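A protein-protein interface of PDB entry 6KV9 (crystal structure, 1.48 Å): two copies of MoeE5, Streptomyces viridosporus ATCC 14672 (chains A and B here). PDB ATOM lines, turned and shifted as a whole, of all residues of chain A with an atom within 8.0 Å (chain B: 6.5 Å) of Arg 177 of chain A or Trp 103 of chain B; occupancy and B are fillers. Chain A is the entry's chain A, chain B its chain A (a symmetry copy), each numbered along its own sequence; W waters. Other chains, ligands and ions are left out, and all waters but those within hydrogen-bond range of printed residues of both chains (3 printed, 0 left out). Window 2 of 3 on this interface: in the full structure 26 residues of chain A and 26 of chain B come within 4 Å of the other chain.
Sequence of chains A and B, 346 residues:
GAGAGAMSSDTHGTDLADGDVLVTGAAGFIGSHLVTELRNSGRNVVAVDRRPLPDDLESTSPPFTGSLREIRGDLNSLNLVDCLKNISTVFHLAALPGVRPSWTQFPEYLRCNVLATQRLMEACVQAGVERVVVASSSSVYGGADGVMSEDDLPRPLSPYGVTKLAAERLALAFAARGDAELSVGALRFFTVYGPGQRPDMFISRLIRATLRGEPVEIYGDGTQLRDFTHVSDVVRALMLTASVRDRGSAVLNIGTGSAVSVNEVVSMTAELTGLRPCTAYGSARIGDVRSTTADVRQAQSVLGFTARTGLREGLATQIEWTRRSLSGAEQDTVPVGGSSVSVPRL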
ATOM      1  N   GLN A 118      -6.062  28.951 -11.497  1.00  0.00           N
ATOM      2  CA  GLN A 118      -6.825  27.884 -10.820  1.00  0.00           C
ATOM      3  C   GLN A 118      -6.401  26.520 -11.331  1.00  0.00           C
ATOM      4  O   GLN A 118      -6.181  25.599 -10.539  1.00  0.00           O
ATOM      5  CB  GLN A 118      -8.297  28.106 -11.125  1.00  0.00           C
ATOM      6  CG  GLN A 118      -9.202  26.969 -10.541  1.00  0.00           C
ATOM      7  CD  GLN A 118      -9.538  25.933 -11.576  1.00  0.00           C
ATOM      8  OE1 GLN A 118      -9.678  26.237 -12.762  1.00  0.00           O
ATOM      9  NE2 GLN A 118      -9.712  24.683 -11.117  1.00  0.00           N
ATOM     10  N   ARG A 119      -6.260  26.393 -12.658  1.00  0.00           N
ATOM     11  CA  ARG A 119      -5.872  25.085 -13.234  1.00  0.00           C
ATOM     12  C   ARG A 119      -4.489  24.672 -12.777  1.00  0.00           C
ATOM     13  O   ARG A 119      -4.256  23.505 -12.407  1.00  0.00           O
ATOM     14  CB  ARG A 119      -5.974  25.135 -14.753  1.00  0.00           C
ATOM     15  CG  ARG A 119      -7.442  25.131 -15.165  1.00  0.00           C
ATOM     16  CD  ARG A 119      -7.628  25.340 -16.640  1.00  0.00           C
ATOM     17  NE  ARG A 119      -9.054  25.101 -16.963  1.00  0.00           N
ATOM     18  CZ  ARG A 119      -9.606  25.411 -18.114  1.00  0.00           C
ATOM     19  NH1 ARG A 119      -8.887  26.092 -19.013  1.00  0.00           N
ATOM     20  NH2 ARG A 119     -10.903  25.116 -18.324  1.00  0.00           N
ATOM     21  N   MET A 121      -2.955  25.647  -9.944  1.00  0.00           N
ATOM     22  CA  MET A 121      -2.936  25.288  -8.542  1.00  0.00           C
ATOM     23  C   MET A 121      -3.554  23.905  -8.302  1.00  0.00           C
ATOM     24  O   MET A 121      -3.049  23.166  -7.451  1.00  0.00           O
ATOM     25  CB  MET A 121      -3.686  26.329  -7.697  1.00  0.00           C
ATOM     26  CG  MET A 121      -3.035  27.768  -7.698  1.00  0.00           C
ATOM     27  SD  MET A 121      -1.311  27.757  -7.196  1.00  0.00           S
ATOM     28  CE  MET A 121      -1.328  26.959  -5.580  1.00  0.00           C
ATOM     29  N   GLU A 122      -4.668  23.595  -8.991  1.00  0.00           N
ATOM     30  CA  GLU A 122      -5.252  22.247  -8.823  1.00  0.00           C
ATOM     31  C   GLU A 122      -4.221  21.192  -9.218  1.00  0.00           C
ATOM     32  O   GLU A 122      -4.038  20.187  -8.492  1.00  0.00           O
ATOM     33  CB  GLU A 122      -6.495  22.160  -9.683  1.00  0.00           C
ATOM     34  CG  GLU A 122      -7.135  20.739  -9.565  1.00  0.00           C
ATOM     35  CD  GLU A 122      -8.407  20.667 -10.317  1.00  0.00           C
ATOM     36  OE1 GLU A 122      -9.459  20.538  -9.675  1.00  0.00           O
ATOM     37  OE2 GLU A 122      -8.352  20.731 -11.553  1.00  0.00           O
ATOM     38  N   VAL A 125      -1.652  20.678  -6.503  1.00  0.00           N
ATOM     39  CA  VAL A 125      -2.138  19.784  -5.438  1.00  0.00           C
ATOM     40  C   VAL A 125      -2.064  18.329  -5.889  1.00  0.00           C
ATOM     41  O   VAL A 125      -1.574  17.455  -5.153  1.00  0.00           O
ATOM     42  CB  VAL A 125      -3.566  20.198  -5.044  1.00  0.00           C
ATOM     43  CG1 VAL A 125      -4.208  19.149  -4.062  1.00  0.00           C
ATOM     44  CG2 VAL A 125      -3.522  21.540  -4.387  1.00  0.00           C
ATOM     45  N   GLN A 126      -2.498  18.060  -7.120  1.00  0.00           N
ATOM     46  CA  GLN A 126      -2.497  16.658  -7.598  1.00  0.00           C
ATOM     47  C   GLN A 126      -1.099  16.089  -7.776  1.00  0.00           C
ATOM     48  O   GLN A 126      -0.887  14.886  -7.565  1.00  0.00           O
ATOM     49  CB  GLN A 126      -3.260  16.560  -8.899  1.00  0.00           C
ATOM     50  CG  GLN A 126      -4.752  16.820  -8.731  1.00  0.00           C
ATOM     51  CD  GLN A 126      -5.444  17.075 -10.044  1.00  0.00           C
ATOM     52  OE1 GLN A 126      -4.915  17.757 -10.944  1.00  0.00           O
ATOM     53  NE2 GLN A 126      -6.665  16.585 -10.178  1.00  0.00           N
ATOM     54  N   LEU A 170      -6.628  33.075  -4.855  1.00  0.00           N
ATOM     55  CA  LEU A 170      -6.875  31.676  -5.218  1.00  0.00           C
ATOM     56  C   LEU A 170      -5.725  30.795  -4.817  1.00  0.00           C
ATOM     57  O   LEU A 170      -5.916  29.677  -4.291  1.00  0.00           O
ATOM     58  CB  LEU A 170      -6.994  31.543  -6.735  1.00  0.00           C
ATOM     59  CG  LEU A 170      -8.290  31.706  -7.458  1.00  0.00           C
ATOM     60  CD1 LEU A 170      -8.010  31.766  -8.958  1.00  0.00           C
ATOM     61  CD2 LEU A 170      -9.209  30.520  -7.111  1.00  0.00           C
ATOM     62  N   ALA A 171      -4.504  31.231  -5.096  1.00  0.00           N
ATOM     63  CA  ALA A 171      -3.350  30.426  -4.721  1.00  0.00           C
ATOM     64  C   ALA A 171      -3.337  30.173  -3.222  1.00  0.00           C
ATOM     65  O   ALA A 171      -3.106  29.031  -2.788  1.00  0.00           O
ATOM     66  CB  ALA A 171      -2.070  31.121  -5.206  1.00  0.00           C
ATOM     67  N   LEU A 172      -3.650  31.196  -2.428  1.00  0.00           N
ATOM     68  CA  LEU A 172      -3.684  31.012  -0.978  1.00  0.00           C
ATOM     69  C   LEU A 172      -4.828  30.095  -0.548  1.00  0.00           C
ATOM     70  O   LEU A 172      -4.659  29.303   0.403  1.00  0.00           O
ATOM     71  CB  LEU A 172      -3.791  32.379  -0.306  1.00  0.00           C
ATOM     72  CG  LEU A 172      -2.525  33.219  -0.475  1.00  0.00           C
ATOM     73  CD1 LEU A 172      -2.834  34.672  -0.134  1.00  0.00           C
ATOM     74  CD2 LEU A 172      -1.347  32.703   0.376  1.00  0.00           C
ATOM     75  N   ALA A 173      -5.973  30.136  -1.230  1.00  0.00           N
ATOM     76  CA  ALA A 173      -7.068  29.203  -0.912  1.00  0.00           C
ATOM     77  C   ALA A 173      -6.640  27.765  -1.171  1.00  0.00           C
ATOM     78  O   ALA A 173      -6.980  26.869  -0.383  1.00  0.00           O
ATOM     79  CB  ALA A 173      -8.304  29.534  -1.747  1.00  0.00           C
ATOM     80  N   PHE A 174      -5.889  27.511  -2.252  1.00  0.00           N
ATOM     81  CA  PHE A 174      -5.439  26.135  -2.483  1.00  0.00           C
ATOM     82  C   PHE A 174      -4.465  25.701  -1.408  1.00  0.00           C
ATOM     83  O   PHE A 174      -4.540  24.564  -0.905  1.00  0.00           O
ATOM     84  CB  PHE A 174      -4.830  25.990  -3.874  1.00  0.00           C
ATOM     85  CG  PHE A 174      -5.847  25.773  -4.979  1.00  0.00           C
ATOM     86  CD1 PHE A 174      -6.466  26.806  -5.616  1.00  0.00           C
ATOM     87  CD2 PHE A 174      -6.191  24.471  -5.328  1.00  0.00           C
ATOM     88  CE1 PHE A 174      -7.425  26.599  -6.605  1.00  0.00           C
ATOM     89  CE2 PHE A 174      -7.120  24.226  -6.309  1.00  0.00           C
ATOM     90  CZ  PHE A 174      -7.740  25.274  -6.986  1.00  0.00           C
ATOM     91  N   ALA A 175      -3.552  26.594  -1.002  1.00  0.00           N
ATOM     92  CA  ALA A 175      -2.588  26.220   0.041  1.00  0.00           C
ATOM     93  C   ALA A 175      -3.272  25.937   1.366  1.00  0.00           C
ATOM     94  O   ALA A 175      -2.747  25.154   2.177  1.00  0.00           O
ATOM     95  CB  ALA A 175      -1.569  27.361   0.210  1.00  0.00           C
ATOM     96  N   ALA A 176      -4.423  26.556   1.602  1.00  0.00           N
ATOM     97  CA  ALA A 176      -5.181  26.361   2.840  1.00  0.00           C
ATOM     98  C   ALA A 176      -5.995  25.067   2.846  1.00  0.00           C
ATOM     99  O   ALA A 176      -6.498  24.705   3.923  1.00  0.00           O
ATOM    100  CB  ALA A 176      -6.108  27.545   3.106  1.00  0.00           C
ATOM    101  N   ARG A 177      -6.168  24.393   1.703  1.00  0.00           N
ATOM    102  CA  ARG A 177      -6.928  23.136   1.703  1.00  0.00           C
ATOM    103  C   ARG A 177      -6.284  22.103   2.620  1.00  0.00           C
ATOM    104  O   ARG A 177      -5.069  21.936   2.645  1.00  0.00           O
ATOM    105  CB  ARG A 177      -6.880  22.563   0.289  1.00  0.00           C
ATOM    106  CG  ARG A 177      -7.652  23.352  -0.777  1.00  0.00           C
ATOM    107  CD  ARG A 177      -7.364  22.787  -2.146  1.00  0.00           C
ATOM    108  NE  ARG A 177      -7.807  21.354  -2.219  1.00  0.00           N
ATOM    109  CZ  ARG A 177      -8.908  20.922  -2.840  1.00  0.00           C
ATOM    110  NH1 ARG A 177      -9.764  21.733  -3.464  1.00  0.00           N
ATOM    111  NH2 ARG A 177      -9.166  19.603  -2.813  1.00  0.00           N
ATOM    112  N   GLY A 178      -7.152  21.332   3.279  1.00  0.00           N
ATOM    113  CA  GLY A 178      -6.623  20.328   4.194  1.00  0.00           C
ATOM    114  C   GLY A 178      -5.881  19.187   3.528  1.00  0.00           C
ATOM    115  O   GLY A 178      -5.123  18.470   4.200  1.00  0.00           O
ATOM    116  N   ASP A 179      -6.092  18.973   2.238  1.00  0.00           N
ATOM    117  CA  ASP A 179      -5.408  17.941   1.493  1.00  0.00           C
ATOM    118  C   ASP A 179      -4.139  18.420   0.817  1.00  0.00           C
ATOM    119  O   ASP A 179      -3.484  17.635   0.130  1.00  0.00           O
ATOM    120  CB  ASP A 179      -6.371  17.280   0.478  1.00  0.00           C
ATOM    121  CG  ASP A 179      -6.806  18.218  -0.647  1.00  0.00           C
ATOM    122  OD1 ASP A 179      -6.632  19.453  -0.515  1.00  0.00           O
ATOM    123  OD2 ASP A 179      -7.333  17.742  -1.668  1.00  0.00           O
ATOM    124  N   ALA A 180      -3.806  19.709   0.935  1.00  0.00           N
ATOM    125  CA  ALA A 180      -2.668  20.282   0.238  1.00  0.00           C
ATOM    126  C   ALA A 180      -1.475  20.243   1.180  1.00  0.00           C
ATOM    127  O   ALA A 180      -1.598  20.549   2.369  1.00  0.00           O
ATOM    128  CB  ALA A 180      -2.955  21.726  -0.190  1.00  0.00           C
ATOM    129  N   GLU A 181      -0.350  19.817   0.649  1.00  0.00           N
ATOM    130  CA  GLU A 181       0.912  19.892   1.359  1.00  0.00           C
ATOM    131  C   GLU A 181       1.746  20.893   0.582  1.00  0.00           C
ATOM    132  O   GLU A 181       2.755  20.554  -0.041  1.00  0.00           O
ATOM    133  CB  GLU A 181       1.570  18.519   1.351  1.00  0.00           C
ATOM    134  CG  GLU A 181       0.543  17.392   1.608  1.00  0.00           C
ATOM    135  CD  GLU A 181       0.972  16.025   1.073  1.00  0.00           C
ATOM    136  OE1 GLU A 181       2.146  15.643   1.267  1.00  0.00           O
ATOM    137  OE2 GLU A 181       0.127  15.336   0.457  1.00  0.00           O
ATOM    138  N   LEU A 182       1.268  22.112   0.533  1.00  0.00           N
ATOM    139  CA  LEU A 182       2.022  23.107  -0.221  1.00  0.00           C
ATOM    140  C   LEU A 182       1.902  24.451   0.446  1.00  0.00           C
ATOM    141  O   LEU A 182       0.881  24.782   1.075  1.00  0.00           O
ATOM    142  CB  LEU A 182       1.768  23.149  -1.733  1.00  0.00           C
ATOM    143  CG  LEU A 182       0.451  23.634  -2.320  1.00  0.00           C
ATOM    144  CD1 LEU A 182       0.335  25.097  -2.217  1.00  0.00           C
ATOM    145  CD2 LEU A 182       0.382  23.214  -3.790  1.00  0.00           C
ATOM    146  N   VAL B  99     -20.999  27.466  -2.610  1.00  0.00           N
ATOM    147  CA  VAL B  99     -19.586  27.415  -2.254  1.00  0.00           C
ATOM    148  C   VAL B  99     -18.885  26.191  -2.844  1.00  0.00           C
ATOM    149  O   VAL B  99     -17.776  26.281  -3.394  1.00  0.00           O
ATOM    150  CB  VAL B  99     -19.429  27.455  -0.716  1.00  0.00           C
ATOM    151  CG1 VAL B  99     -18.010  27.079  -0.299  1.00  0.00           C
ATOM    152  CG2 VAL B  99     -19.883  28.840  -0.191  1.00  0.00           C
ATOM    153  N   ARG B 100     -19.482  24.999  -2.668  1.00  0.00           N
ATOM    154  CA  ARG B 100     -18.740  23.759  -2.876  1.00  0.00           C
ATOM    155  C   ARG B 100     -18.495  23.361  -4.332  1.00  0.00           C
ATOM    156  O   ARG B 100     -17.374  22.910  -4.655  1.00  0.00           O
ATOM    157  CB  ARG B 100     -19.394  22.651  -2.020  1.00  0.00           C
ATOM    158  CG  ARG B 100     -19.219  22.973  -0.524  1.00  0.00           C
ATOM    159  CD  ARG B 100     -20.074  22.066   0.403  1.00  0.00           C
ATOM    160  NE  ARG B 100     -21.493  22.400   0.245  1.00  0.00           N
ATOM    161  CZ  ARG B 100     -22.120  23.386   0.876  1.00  0.00           C
ATOM    162  NH1 ARG B 100     -21.436  24.170   1.730  1.00  0.00           N
ATOM    163  NH2 ARG B 100     -23.404  23.604   0.676  1.00  0.00           N
ATOM    164  N   PRO B 101     -19.441  23.588  -5.250  1.00  0.00           N
ATOM    165  CA  PRO B 101     -19.199  23.246  -6.670  1.00  0.00           C
ATOM    166  C   PRO B 101     -18.169  24.134  -7.337  1.00  0.00           C
ATOM    167  O   PRO B 101     -17.716  23.855  -8.446  1.00  0.00           O
ATOM    168  CB  PRO B 101     -20.565  23.451  -7.325  1.00  0.00           C
ATOM    169  CG  PRO B 101     -21.547  23.248  -6.192  1.00  0.00           C
ATOM    170  CD  PRO B 101     -20.865  23.869  -5.004  1.00  0.00           C
ATOM    171  N   SER B 102     -17.809  25.246  -6.710  1.00  0.00           N
ATOM    172  CA  SER B 102     -16.899  26.168  -7.376  1.00  0.00           C
ATOM    173  C   SER B 102     -15.511  25.591  -7.638  1.00  0.00           C
ATOM    174  O   SER B 102     -14.805  26.113  -8.516  1.00  0.00           O
ATOM    175  CB  SER B 102     -16.807  27.438  -6.510  1.00  0.00           C
ATOM    176  OG  SER B 102     -16.080  27.216  -5.322  1.00  0.00           O
ATOM    177  N   TRP B 103     -15.070  24.553  -6.916  1.00  0.00           N
ATOM    178  CA  TRP B 103     -13.776  23.977  -7.260  1.00  0.00           C
ATOM    179  C   TRP B 103     -13.793  23.286  -8.618  1.00  0.00           C
ATOM    180  O   TRP B 103     -12.752  23.249  -9.313  1.00  0.00           O
ATOM    181  CB  TRP B 103     -13.390  22.902  -6.246  1.00  0.00           C
ATOM    182  CG  TRP B 103     -13.195  23.370  -4.845  1.00  0.00           C
ATOM    183  CD1 TRP B 103     -14.077  23.211  -3.794  1.00  0.00           C
ATOM    184  CD2 TRP B 103     -12.058  24.059  -4.306  1.00  0.00           C
ATOM    185  NE1 TRP B 103     -13.550  23.749  -2.630  1.00  0.00           N
ATOM    186  CE2 TRP B 103     -12.305  24.246  -2.912  1.00  0.00           C
ATOM    187  CE3 TRP B 103     -10.839  24.509  -4.838  1.00  0.00           C
ATOM    188  CZ2 TRP B 103     -11.414  24.897  -2.078  1.00  0.00           C
ATOM    189  CZ3 TRP B 103      -9.911  25.151  -3.980  1.00  0.00           C
ATOM    190  CH2 TRP B 103     -10.212  25.350  -2.621  1.00  0.00           C
ATOM    191  N   THR B 104     -14.934  22.692  -8.994  1.00  0.00           N
ATOM    192  CA  THR B 104     -14.974  21.849 -10.184  1.00  0.00           C
ATOM    193  C   THR B 104     -15.774  22.446 -11.327  1.00  0.00           C
ATOM    194  O   THR B 104     -15.871  21.833 -12.392  1.00  0.00           O
ATOM    195  CB  THR B 104     -15.481  20.439  -9.824  1.00  0.00           C
ATOM    196  OG1 THR B 104     -16.781  20.572  -9.223  1.00  0.00           O
ATOM    197  CG2 THR B 104     -14.527  19.809  -8.851  1.00  0.00           C
ATOM    198  N   GLN B 105     -16.293  23.655 -11.177  1.00  0.00           N
ATOM    199  CA  GLN B 105     -17.067  24.369 -12.167  1.00  0.00           C
ATOM    200  C   GLN B 105     -16.491  25.777 -12.347  1.00  0.00           C
ATOM    201  O   GLN B 105     -17.221  26.727 -12.577  1.00  0.00           O
ATOM    202  CB  GLN B 105     -18.535  24.451 -11.760  1.00  0.00           C
ATOM    203  CG  GLN B 105     -19.228  23.046 -11.705  1.00  0.00           C
ATOM    204  CD  GLN B 105     -20.624  23.139 -11.139  1.00  0.00           C
ATOM    205  OE1 GLN B 105     -21.196  24.227 -10.985  1.00  0.00           O
ATOM    206  NE2 GLN B 105     -21.176  21.992 -10.796  1.00  0.00           N
ATOM    207  N   PHE B 106     -15.181  25.892 -12.180  1.00  0.00           N
ATOM    208  CA  PHE B 106     -14.623  27.236 -12.101  1.00  0.00           C
ATOM    209  C   PHE B 106     -14.816  28.094 -13.352  1.00  0.00           C
ATOM    210  O   PHE B 106     -15.120  29.297 -13.206  1.00  0.00           O
ATOM    211  CB  PHE B 106     -13.181  27.175 -11.644  1.00  0.00           C
ATOM    212  CG  PHE B 106     -12.658  28.518 -11.174  1.00  0.00           C
ATOM    213  CD1 PHE B 106     -13.279  29.207 -10.105  1.00  0.00           C
ATOM    214  CD2 PHE B 106     -11.546  29.082 -11.803  1.00  0.00           C
ATOM    215  CE1 PHE B 106     -12.763  30.452  -9.676  1.00  0.00           C
ATOM    216  CE2 PHE B 106     -11.061  30.325 -11.389  1.00  0.00           C
ATOM    217  CZ  PHE B 106     -11.652  31.020 -10.330  1.00  0.00           C
ATOM    218  N   TYR B 109     -18.204  29.622 -12.933  1.00  0.00           N
ATOM    219  CA  TYR B 109     -18.242  30.614 -11.851  1.00  0.00           C
ATOM    220  C   TYR B 109     -17.570  31.925 -12.274  1.00  0.00           C
ATOM    221  O   TYR B 109     -18.066  33.000 -11.958  1.00  0.00           O
ATOM    222  CB  TYR B 109     -17.588  30.030 -10.594  1.00  0.00           C
ATOM    223  CG  TYR B 109     -18.519  29.211  -9.753  1.00  0.00           C
ATOM    224  CD1 TYR B 109     -18.938  27.946 -10.150  1.00  0.00           C
ATOM    225  CD2 TYR B 109     -18.928  29.693  -8.527  1.00  0.00           C
ATOM    226  CE1 TYR B 109     -19.795  27.202  -9.340  1.00  0.00           C
ATOM    227  CE2 TYR B 109     -19.798  28.952  -7.697  1.00  0.00           C
ATOM    228  CZ  TYR B 109     -20.195  27.703  -8.119  1.00  0.00           C
ATOM    229  OH  TYR B 109     -21.039  26.955  -7.330  1.00  0.00           O
ATOM    230  N   LEU B 157     -11.491  31.041   1.239  1.00  0.00           N
ATOM    231  CA  LEU B 157     -11.000  29.670   1.230  1.00  0.00           C
ATOM    232  C   LEU B 157     -11.640  28.825   0.127  1.00  0.00           C
ATOM    233  O   LEU B 157     -11.296  27.641   0.003  1.00  0.00           O
ATOM    234  CB  LEU B 157     -11.276  29.023   2.604  1.00  0.00           C
ATOM    235  CG  LEU B 157     -10.444  29.652   3.722  1.00  0.00           C
ATOM    236  CD1 LEU B 157     -10.701  28.874   5.011  1.00  0.00           C
ATOM    237  CD2 LEU B 157      -8.979  29.641   3.373  1.00  0.00           C
ATOM    238  N   SER B 158     -12.555  29.371  -0.666  1.00  0.00           N
ATOM    239  CA  SER B 158     -13.126  28.658  -1.812  1.00  0.00           C
ATOM    240  C   SER B 158     -12.984  29.494  -3.077  1.00  0.00           C
ATOM    241  O   SER B 158     -12.957  30.743  -3.019  1.00  0.00           O
ATOM    242  CB  SER B 158     -14.615  28.360  -1.613  1.00  0.00           C
ATOM    243  OG  SER B 158     -15.367  29.563  -1.444  1.00  0.00           O
ATOM    244  N   PRO B 159     -12.938  28.857  -4.246  1.00  0.00           N
ATOM    245  CA  PRO B 159     -12.970  29.649  -5.500  1.00  0.00           C
ATOM    246  C   PRO B 159     -14.218  30.517  -5.598  1.00  0.00           C
ATOM    247  O   PRO B 159     -14.141  31.638  -6.115  1.00  0.00           O
ATOM    248  CB  PRO B 159     -12.912  28.575  -6.611  1.00  0.00           C
ATOM    249  CG  PRO B 159     -12.211  27.393  -5.931  1.00  0.00           C
ATOM    250  CD  PRO B 159     -12.743  27.403  -4.503  1.00  0.00           C
ATOM    251  N   TYR B 160     -15.370  30.077  -5.096  1.00  0.00           N
ATOM    252  CA  TYR B 160     -16.552  30.925  -5.044  1.00  0.00           C
ATOM    253  C   TYR B 160     -16.255  32.218  -4.296  1.00  0.00           C
ATOM    254  O   TYR B 160     -16.571  33.312  -4.776  1.00  0.00           O
ATOM    255  CB  TYR B 160     -17.728  30.170  -4.358  1.00  0.00           C
ATOM    256  CG  TYR B 160     -18.877  31.050  -4.004  1.00  0.00           C
ATOM    257  CD1 TYR B 160     -19.703  31.613  -4.984  1.00  0.00           C
ATOM    258  CD2 TYR B 160     -19.121  31.412  -2.662  1.00  0.00           C
ATOM    259  CE1 TYR B 160     -20.776  32.418  -4.669  1.00  0.00           C
ATOM    260  CE2 TYR B 160     -20.202  32.251  -2.357  1.00  0.00           C
ATOM    261  CZ  TYR B 160     -21.030  32.751  -3.340  1.00  0.00           C
ATOM    262  OH  TYR B 160     -22.114  33.519  -3.034  1.00  0.00           O
ATOM    263  N   ARG B 285     -16.318  19.150   3.807  1.00  0.00           N
ATOM    264  CA  ARG B 285     -16.089  19.511   2.406  1.00  0.00           C
ATOM    265  C   ARG B 285     -15.068  20.637   2.340  1.00  0.00           C
ATOM    266  O   ARG B 285     -15.306  21.732   2.885  1.00  0.00           O
ATOM    267  CB  ARG B 285     -17.379  19.945   1.727  1.00  0.00           C
ATOM    268  CG  ARG B 285     -18.442  18.824   1.611  1.00  0.00           C
ATOM    269  CD  ARG B 285     -18.019  17.744   0.628  1.00  0.00           C
ATOM    270  NE  ARG B 285     -19.176  16.938   0.157  1.00  0.00           N
ATOM    271  CZ  ARG B 285     -19.633  15.822   0.731  1.00  0.00           C
ATOM    272  NH1 ARG B 285     -19.087  15.343   1.838  1.00  0.00           N
ATOM    273  NH2 ARG B 285     -20.671  15.187   0.196  1.00  0.00           N
ATOM    274  N   ILE B 286     -13.947  20.361   1.665  1.00  0.00           N
ATOM    275  CA  ILE B 286     -12.902  21.374   1.486  1.00  0.00           C
ATOM    276  C   ILE B 286     -13.484  22.642   0.855  1.00  0.00           C
ATOM    277  O   ILE B 286     -14.274  22.608  -0.088  1.00  0.00           O
ATOM    278  CB  ILE B 286     -11.749  20.755   0.687  1.00  0.00           C
ATOM    279  CG1 ILE B 286     -11.060  19.628   1.526  1.00  0.00           C
ATOM    280  CG2 ILE B 286     -10.711  21.848   0.275  1.00  0.00           C
ATOM    281  CD1 ILE B 286      -9.861  19.049   0.891  1.00  0.00           C
ATOM    282  N   GLY B 287     -13.164  23.773   1.471  1.00  0.00           N
ATOM    283  CA  GLY B 287     -13.675  25.064   1.040  1.00  0.00           C
ATOM    284  C   GLY B 287     -14.717  25.636   1.975  1.00  0.00           C
ATOM    285  O   GLY B 287     -14.930  26.854   1.971  1.00  0.00           O
ATOM    286  N   ASP B 288     -15.408  24.789   2.748  1.00  0.00           N
ATOM    287  CA  ASP B 288     -16.343  25.296   3.745  1.00  0.00           C
ATOM    288  C   ASP B 288     -15.583  25.874   4.926  1.00  0.00           C
ATOM    289  O   ASP B 288     -14.721  25.208   5.530  1.00  0.00           O
ATOM    290  CB  ASP B 288     -17.185  24.137   4.307  1.00  0.00           C
ATOM    291  CG  ASP B 288     -18.354  23.737   3.418  1.00  0.00           C
ATOM    292  OD1 ASP B 288     -18.724  24.440   2.471  1.00  0.00           O
ATOM    293  OD2 ASP B 288     -18.954  22.648   3.703  1.00  0.00           O
HETATM  294  O   HOH W   1      -9.234  26.075   1.099  1.00  0.00           O
HETATM  295  O   HOH W   2     -10.406  24.172  -8.387  1.00  0.00           O
HETATM  296  O   HOH W   3     -11.291  22.160 -11.367  1.00  0.00           O
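Among the printed residues, pairs that only touch across the chains: Arg 177 of chain A with Trp 103 of chain B, Gln 118 of chain A with Phe 106 of chain B, Asp 179 of chain A with Ile 286 of chain B, Ala 176 of chain A with Leu 157 of chain B, Arg 177 of chain A with Ile 286 of chain B, Phe 174 of chain A with Trp 103 of chain B, Gln 118 of chain A with Trp 103 of chain B, Ala 173 of chain A with Leu 157 of chain B and Leu 170 of chain A with Phe 106 of chain B.
The indole nitrogen (NE1) of Trp 103 of chain B lies within hydrogen-bond range of the backbone carbonyl oxygen (O) of Ile 286 of chain B (2.9 Å). The guanidinium group of Arg 177 of chain A is in salt-bridge range of the side-chain carboxylate of Asp 179 of chain A (2.8 Å).
Of the 17 printed residues of chain B, 4 touch a printed residue of chain A. Of the 19 printed residues of chain A, 7 touch a printed residue of chain B. Among the printed residues, 9 pairs touch across the chains. Among the printed residues, no Asp or Glu carboxylate lies within 4 Å of a Lys or Arg side-chain nitrogen of the other chain.
No position is printed for both chains. Of the 9 pairs that touch across the chains among the printed residues, none has its exchanged pair printed and touching as well.
Of chain B, only Trp 103 (3.3 Å) and Ile 286 (3.6 Å) come within 4 Å of Arg 177 of chain A. Trp 103 of chain B touches three residues of chain A. No residue of chain A comes within 4 Å of Ser 102 of chain B. Of the printed residues of chain B, Asp 179 of chain A touches Ile 286. Printed residues of chain B within 4 Å of Ala 173 of chain A: Leu 157. Printed residues of chain B within 4 Å of Leu 170 of chain A: Phe 106. Of the printed residues of chain B, Phe 174 of chain A touches Trp 103. Arg 100 of chain B touches none of the printed residues of chain A. The nearest printed residue of chain B that does not touch Leu 170 of chain A is Pro 159 of chain B (4.2 Å).
Water W2 lies within hydrogen-bond range of the backbone carbonyl oxygen (O) of Trp 103 of chain B and the side-chain amide nitrogen (NE2) of Gln 118 of chain A. Water W3 lies within hydrogen-bond range of the backbone carbonyl oxygen of Trp 103 of chain B, the side-chain carboxylate of Glu 122 of chain A and the side-chain amide nitrogen of Gln 118 of chain A. Water W1 lies within hydrogen-bond range of O of Leu 157 of chain B (2.8 Å) and O of Ala 173 of chain A (2.8 Å).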
